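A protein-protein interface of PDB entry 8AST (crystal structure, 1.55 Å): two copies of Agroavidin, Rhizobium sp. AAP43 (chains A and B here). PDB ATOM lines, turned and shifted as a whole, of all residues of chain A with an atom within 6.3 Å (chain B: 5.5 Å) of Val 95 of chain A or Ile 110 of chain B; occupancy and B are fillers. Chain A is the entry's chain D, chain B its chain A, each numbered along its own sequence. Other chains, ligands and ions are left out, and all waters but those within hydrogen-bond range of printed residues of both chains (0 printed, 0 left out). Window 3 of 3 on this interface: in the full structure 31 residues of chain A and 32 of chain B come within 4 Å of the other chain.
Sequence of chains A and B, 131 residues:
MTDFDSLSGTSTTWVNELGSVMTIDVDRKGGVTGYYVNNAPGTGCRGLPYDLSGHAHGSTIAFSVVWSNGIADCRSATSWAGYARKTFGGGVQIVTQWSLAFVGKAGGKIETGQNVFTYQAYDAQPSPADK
The side-chain amide nitrogen (NE2) of Gln 97 of chain A lies close to the side-chain amide nitrogen (NE2) of Gln 114 of chain A (2.8 Å). N of Lys 109 of chain B lies within hydrogen-bond range of O of Phe 102 of chain B (2.8 Å). O of Ala 81 of chain A lies within hydrogen-bond range of N of Gln 97 of chain A (2.9 Å). O of Tyr 83 of chain A sits at hydrogen-bond distance from N of Val 95 of chain A (2.9 Å). The side-chain hydroxyl (OG1) of Thr 96 of chain A is in hydrogen-bond range of the backbone carbonyl oxygen (O) of Asn 115 of chain A, 2.7 Å away.
C of Ala 81 of chain A touches CB of Ala 101 of chain B, at 3.8 Å. CD1 of Ile 110 of chain B touches O of Ala 81 of chain A, 3.9 Å away. C of Gly 82 of chain A touches CB of Ala 101 of chain B (3.5 Å). Tyr 83 of chain A touches Gly 108 of chain B (CE2 to C, 3.5 Å). CE2 of Tyr 83 of chain A touches N of Lys 109 of chain B (3.7 Å). O of Val 95 of chain A touches CD1 of Ile 110 of chain B, 3.7 Å away. Ile 110 of chain B touches Thr 96 of chain A (CD1 to C, 3.4 Å). CB of Gln 97 of chain A touches CG2 of Ile 110 of chain B, at 3.2 Å.
Of chain B, only Ile 110 (3.7 Å) comes within 4 Å of Val 95 of chain A. Val 116 of chain A touches none of the printed residues of chain B. Printed residues of chain A within 4 Å of Ala 101 of chain B: Ala 81 and Gly 82. Of the printed residues of chain A, Gly 108 of chain B touches Tyr 83 (3.5 Å). The nearest residue of chain A that does not touch Ile 110 of chain B is Tyr 83 of chain A (4.3 Å).
Of the 8 printed residues of chain B, 4 touch a printed residue of chain A. Printed residues of chain B that touch a printed residue of chain A: Ala 101, Gly 108, Lys 109 and Ile 110. Hydrophobic or aromatic side chains of chain B within 4 Å of the printed part of chain A: Ala 101 and Ile 110. Among the printed residues, 8 pairs touch across the chains. Among the printed residues, no Asp or Glu carboxylate lies within 4 Å of a Lys or Arg side-chain nitrogen of the other chain.
No position is printed for both chains.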
ATOM      1  N   ALA A  81      12.418  22.410  -6.545  1.00  0.00           N
ATOM      2  CA  ALA A  81      11.368  23.395  -6.272  1.00  0.00           C
ATOM      3  C   ALA A  81      11.029  24.080  -7.596  1.00  0.00           C
ATOM      4  O   ALA A  81      11.957  24.418  -8.338  1.00  0.00           O
ATOM      5  CB  ALA A  81      11.806  24.413  -5.246  1.00  0.00           C
ATOM      6  N   GLY A  82       9.754  24.293  -7.866  1.00  0.00           N
ATOM      7  CA  GLY A  82       9.371  24.871  -9.160  1.00  0.00           C
ATOM      8  C   GLY A  82       8.098  25.640  -9.146  1.00  0.00           C
ATOM      9  O   GLY A  82       7.336  25.608  -8.144  1.00  0.00           O
ATOM     10  N   TYR A  83       7.895  26.387 -10.228  1.00  0.00           N
ATOM     11  CA  TYR A  83       6.640  27.121 -10.460  1.00  0.00           C
ATOM     12  C   TYR A  83       6.012  26.691 -11.784  1.00  0.00           C
ATOM     13  O   TYR A  83       6.742  26.241 -12.713  1.00  0.00           O
ATOM     14  CB  TYR A  83       6.859  28.618 -10.384  1.00  0.00           C
ATOM     15  CG  TYR A  83       7.810  29.156 -11.408  1.00  0.00           C
ATOM     16  CD1 TYR A  83       7.321  29.565 -12.638  1.00  0.00           C
ATOM     17  CD2 TYR A  83       9.159  29.304 -11.147  1.00  0.00           C
ATOM     18  CE1 TYR A  83       8.163  30.079 -13.599  1.00  0.00           C
ATOM     19  CE2 TYR A  83      10.018  29.842 -12.097  1.00  0.00           C
ATOM     20  CZ  TYR A  83       9.509  30.209 -13.338  1.00  0.00           C
ATOM     21  OH  TYR A  83      10.346  30.760 -14.264  1.00  0.00           O
ATOM     22  N   ALA A  84       4.686  26.812 -11.844  1.00  0.00           N
ATOM     23  CA  ALA A  84       3.892  26.503 -13.049  1.00  0.00           C
ATOM     24  C   ALA A  84       4.044  27.675 -14.036  1.00  0.00           C
ATOM     25  O   ALA A  84       4.018  28.859 -13.623  1.00  0.00           O
ATOM     26  CB  ALA A  84       2.449  26.252 -12.694  1.00  0.00           C
ATOM     27  N   ARG A  85       4.293  27.374 -15.310  1.00  0.00           N
ATOM     28  CA  ARG A  85       4.402  28.410 -16.380  1.00  0.00           C
ATOM     29  C   ARG A  85       3.505  27.979 -17.539  1.00  0.00           C
ATOM     30  O   ARG A  85       3.726  26.896 -18.127  1.00  0.00           O
ATOM     31  CB  ARG A  85       5.877  28.614 -16.747  1.00  0.00           C
ATOM     32  CG  ARG A  85       6.121  29.795 -17.691  1.00  0.00           C
ATOM     33  CD  ARG A  85       7.564  29.947 -18.107  1.00  0.00           C
ATOM     34  NE  ARG A  85       8.023  28.799 -18.896  1.00  0.00           N
ATOM     35  CZ  ARG A  85       9.290  28.517 -19.098  1.00  0.00           C
ATOM     36  NH1 ARG A  85       9.622  27.439 -19.769  1.00  0.00           N
ATOM     37  NH2 ARG A  85      10.247  29.274 -18.584  1.00  0.00           N
ATOM     38  N   GLN A  93       4.150  24.087 -18.055  1.00  0.00           N
ATOM     39  CA  GLN A  93       5.469  23.503 -17.756  1.00  0.00           C
ATOM     40  C   GLN A  93       5.748  23.745 -16.275  1.00  0.00           C
ATOM     41  O   GLN A  93       5.186  24.685 -15.663  1.00  0.00           O
ATOM     42  CB  GLN A  93       6.595  24.141 -18.576  1.00  0.00           C
ATOM     43  CG  GLN A  93       6.511  23.749 -20.042  1.00  0.00           C
ATOM     44  CD  GLN A  93       7.595  24.397 -20.860  1.00  0.00           C
ATOM     45  OE1 GLN A  93       7.754  25.609 -20.841  1.00  0.00           O
ATOM     46  NE2 GLN A  93       8.304  23.588 -21.635  1.00  0.00           N
ATOM     47  N   ILE A  94       6.606  22.913 -15.732  1.00  0.00           N
ATOM     48  CA  ILE A  94       7.148  23.151 -14.363  1.00  0.00           C
ATOM     49  C   ILE A  94       8.596  23.587 -14.516  1.00  0.00           C
ATOM     50  O   ILE A  94       9.444  22.777 -14.974  1.00  0.00           O
ATOM     51  CB  ILE A  94       7.017  21.902 -13.497  1.00  0.00           C
ATOM     52  CG1 ILE A  94       5.638  21.264 -13.571  1.00  0.00           C
ATOM     53  CG2 ILE A  94       7.436  22.251 -12.076  1.00  0.00           C
ATOM     54  CD1 ILE A  94       5.544  19.937 -12.817  1.00  0.00           C
ATOM     55  N   VAL A  95       8.865  24.829 -14.146  1.00  0.00           N
ATOM     56  CA  VAL A  95      10.214  25.420 -14.198  1.00  0.00           C
ATOM     57  C   VAL A  95      10.844  25.165 -12.832  1.00  0.00           C
ATOM     58  O   VAL A  95      10.306  25.706 -11.855  1.00  0.00           O
ATOM     59  CB  VAL A  95      10.194  26.912 -14.522  1.00  0.00           C
ATOM     60  CG1 VAL A  95      11.601  27.478 -14.462  1.00  0.00           C
ATOM     61  CG2 VAL A  95       9.556  27.138 -15.879  1.00  0.00           C
ATOM     62  N   THR A  96      11.886  24.340 -12.765  1.00  0.00           N
ATOM     63  CA  THR A  96      12.482  23.921 -11.460  1.00  0.00           C
ATOM     64  C   THR A  96      13.940  24.340 -11.333  1.00  0.00           C
ATOM     65  O   THR A  96      14.692  24.492 -12.361  1.00  0.00           O
ATOM     66  CB  THR A  96      12.387  22.409 -11.216  1.00  0.00           C
ATOM     67  OG1 THR A  96      13.298  21.724 -12.078  1.00  0.00           O
ATOM     68  CG2 THR A  96      10.999  21.854 -11.401  1.00  0.00           C
ATOM     69  N   GLN A  97      14.339  24.430 -10.070  1.00  0.00           N
ATOM     70  CA  GLN A  97      15.748  24.433  -9.652  1.00  0.00           C
ATOM     71  C   GLN A  97      15.881  23.195  -8.789  1.00  0.00           C
ATOM     72  O   GLN A  97      15.019  22.988  -7.940  1.00  0.00           O
ATOM     73  CB  GLN A  97      16.082  25.713  -8.894  1.00  0.00           C
ATOM     74  CG  GLN A  97      17.524  25.844  -8.421  1.00  0.00           C
ATOM     75  CD  GLN A  97      18.465  26.289  -9.520  1.00  0.00           C
ATOM     76  OE1 GLN A  97      19.681  26.146  -9.407  1.00  0.00           O
ATOM     77  NE2 GLN A  97      17.907  26.741 -10.631  1.00  0.00           N
ATOM     78  N   GLN A 114      19.165  23.611 -13.185  1.00  0.00           N
ATOM     79  CA  GLN A 114      17.796  23.930 -13.628  1.00  0.00           C
ATOM     80  C   GLN A 114      17.273  22.776 -14.467  1.00  0.00           C
ATOM     81  O   GLN A 114      18.081  22.153 -15.195  1.00  0.00           O
ATOM     82  CB  GLN A 114      17.762  25.197 -14.489  1.00  0.00           C
ATOM     83  CG  GLN A 114      18.013  26.463 -13.704  1.00  0.00           C
ATOM     84  CD  GLN A 114      19.470  26.842 -13.664  1.00  0.00           C
ATOM     85  OE1 GLN A 114      20.120  26.937 -14.705  1.00  0.00           O
ATOM     86  NE2 GLN A 114      19.988  27.077 -12.462  1.00  0.00           N
ATOM     87  N   ASN A 115      15.970  22.508 -14.374  1.00  0.00           N
ATOM     88  CA  ASN A 115      15.256  21.502 -15.184  1.00  0.00           C
ATOM     89  C   ASN A 115      13.884  22.092 -15.502  1.00  0.00           C
ATOM     90  O   ASN A 115      13.261  22.609 -14.605  1.00  0.00           O
ATOM     91  CB  ASN A 115      14.924  20.169 -14.487  1.00  0.00           C
ATOM     92  CG  ASN A 115      16.019  19.117 -14.305  1.00  0.00           C
ATOM     93  OD1 ASN A 115      15.821  18.148 -13.520  1.00  0.00           O
ATOM     94  ND2 ASN A 115      17.144  19.280 -15.001  1.00  0.00           N
ATOM     95  N   VAL A 116      13.434  22.002 -16.754  1.00  0.00           N
ATOM     96  CA  VAL A 116      12.042  22.346 -17.127  1.00  0.00           C
ATOM     97  C   VAL A 116      11.325  21.070 -17.534  1.00  0.00           C
ATOM     98  O   VAL A 116      11.785  20.345 -18.452  1.00  0.00           O
ATOM     99  CB  VAL A 116      11.997  23.413 -18.234  1.00  0.00           C
ATOM    100  CG1 VAL A 116      10.570  23.684 -18.664  1.00  0.00           C
ATOM    101  CG2 VAL A 116      12.690  24.701 -17.811  1.00  0.00           C
ATOM    102  N   PHE A 117      10.195  20.812 -16.900  1.00  0.00           N
ATOM    103  CA  PHE A 117       9.367  19.623 -17.142  1.00  0.00           C
ATOM    104  C   PHE A 117       8.153  20.023 -17.990  1.00  0.00           C
ATOM    105  O   PHE A 117       7.473  20.991 -17.685  1.00  0.00           O
ATOM    106  CB  PHE A 117       8.903  19.010 -15.827  1.00  0.00           C
ATOM    107  CG  PHE A 117      10.013  18.360 -15.045  1.00  0.00           C
ATOM    108  CD1 PHE A 117      10.782  19.114 -14.195  1.00  0.00           C
ATOM    109  CD2 PHE A 117      10.320  17.007 -15.186  1.00  0.00           C
ATOM    110  CE1 PHE A 117      11.808  18.528 -13.455  1.00  0.00           C
ATOM    111  CE2 PHE A 117      11.380  16.436 -14.496  1.00  0.00           C
ATOM    112  CZ  PHE A 117      12.130  17.208 -13.626  1.00  0.00           C
ATOM    113  N   LEU B 100      14.535  27.619  -3.966  1.00  0.00           N
ATOM    114  CA  LEU B 100      13.279  28.294  -3.585  1.00  0.00           C
ATOM    115  C   LEU B 100      12.592  28.752  -4.870  1.00  0.00           C
ATOM    116  O   LEU B 100      13.261  29.476  -5.652  1.00  0.00           O
ATOM    117  CB  LEU B 100      13.607  29.463  -2.659  1.00  0.00           C
ATOM    118  CG  LEU B 100      12.521  30.521  -2.493  1.00  0.00           C
ATOM    119  CD1 LEU B 100      11.279  29.958  -1.874  1.00  0.00           C
ATOM    120  CD2 LEU B 100      13.026  31.690  -1.665  1.00  0.00           C
ATOM    121  N   ALA B 101      11.331  28.387  -5.065  1.00  0.00           N
ATOM    122  CA  ALA B 101      10.547  28.867  -6.226  1.00  0.00           C
ATOM    123  C   ALA B 101       9.427  29.737  -5.681  1.00  0.00           C
ATOM    124  O   ALA B 101       8.771  29.327  -4.706  1.00  0.00           O
ATOM    125  CB  ALA B 101      10.010  27.727  -7.047  1.00  0.00           C
ATOM    126  N   PHE B 102       9.234  30.925  -6.235  1.00  0.00           N
ATOM    127  CA  PHE B 102       8.123  31.789  -5.775  1.00  0.00           C
ATOM    128  C   PHE B 102       7.479  32.534  -6.937  1.00  0.00           C
ATOM    129  O   PHE B 102       8.064  32.561  -8.040  1.00  0.00           O
ATOM    130  CB  PHE B 102       8.587  32.726  -4.674  1.00  0.00           C
ATOM    131  CG  PHE B 102       9.674  33.707  -5.002  1.00  0.00           C
ATOM    132  CD1 PHE B 102      11.013  33.334  -4.956  1.00  0.00           C
ATOM    133  CD2 PHE B 102       9.356  35.029  -5.276  1.00  0.00           C
ATOM    134  CE1 PHE B 102      12.018  34.241  -5.247  1.00  0.00           C
ATOM    135  CE2 PHE B 102      10.365  35.940  -5.543  1.00  0.00           C
ATOM    136  CZ  PHE B 102      11.690  35.546  -5.529  1.00  0.00           C
ATOM    137  N   GLY B 108       7.166  34.044 -12.003  1.00  0.00           N
ATOM    138  CA  GLY B 108       7.892  32.938 -11.338  1.00  0.00           C
ATOM    139  C   GLY B 108       9.382  33.207 -11.254  1.00  0.00           C
ATOM    140  O   GLY B 108       9.979  33.641 -12.259  1.00  0.00           O
ATOM    141  N   LYS B 109       9.990  32.973 -10.091  1.00  0.00           N
ATOM    142  CA  LYS B 109      11.441  33.194  -9.883  1.00  0.00           C
ATOM    143  C   LYS B 109      12.004  32.017  -9.094  1.00  0.00           C
ATOM    144  O   LYS B 109      11.234  31.424  -8.353  1.00  0.00           O
ATOM    145  CB  LYS B 109      11.707  34.489  -9.120  1.00  0.00           C
ATOM    146  CG  LYS B 109      11.742  35.732  -9.992  1.00  0.00           C
ATOM    147  CD  LYS B 109      13.160  36.147 -10.364  1.00  0.00           C
ATOM    148  CE  LYS B 109      13.292  36.736 -11.757  1.00  0.00           C
ATOM    149  NZ  LYS B 109      12.589  38.037 -11.867  1.00  0.00           N
ATOM    150  N   ILE B 110      13.297  31.780  -9.209  1.00  0.00           N
ATOM    151  CA  ILE B 110      13.994  30.728  -8.427  1.00  0.00           C
ATOM    152  C   ILE B 110      15.225  31.317  -7.750  1.00  0.00           C
ATOM    153  O   ILE B 110      15.954  32.084  -8.403  1.00  0.00           O
ATOM    154  CB  ILE B 110      14.306  29.552  -9.362  1.00  0.00           C
ATOM    155  CG1 ILE B 110      13.100  28.622  -9.430  1.00  0.00           C
ATOM    156  CG2 ILE B 110      15.579  28.848  -8.934  1.00  0.00           C
ATOM    157  CD1 ILE B 110      13.232  27.507 -10.417  1.00  0.00           C
ATOM    158  N   GLU B 111      15.429  31.005  -6.466  1.00  0.00           N
ATOM    159  CA  GLU B 111      16.652  31.409  -5.714  1.00  0.00           C
ATOM    160  C   GLU B 111      17.284  30.153  -5.142  1.00  0.00           C
ATOM    161  O   GLU B 111      16.552  29.163  -4.971  1.00  0.00           O
ATOM    162  CB  GLU B 111      16.334  32.352  -4.568  1.00  0.00           C
ATOM    163  CG  GLU B 111      15.913  33.728  -5.016  1.00  0.00           C
ATOM    164  CD  GLU B 111      15.380  34.582  -3.887  1.00  0.00           C
ATOM    165  OE1 GLU B 111      15.553  34.186  -2.719  1.00  0.00           O
ATOM    166  OE2 GLU B 111      14.788  35.639  -4.181  1.00  0.00           O
ATOM    167  N   THR B 112      18.582  30.191  -4.847  1.00  0.00           N
ATOM    168  CA  THR B 112      19.302  29.015  -4.315  1.00  0.00           C
ATOM    169  C   THR B 112      20.248  29.497  -3.220  1.00  0.00           C
ATOM    170  O   THR B 112      20.620  30.689  -3.196  1.00  0.00           O
ATOM    171  CB  THR B 112      20.003  28.256  -5.445  1.00  0.00           C
ATOM    172  OG1 THR B 112      20.489  26.979  -5.000  1.00  0.00           O
ATOM    173  CG2 THR B 112      21.153  29.078  -5.991  1.00  0.00           C
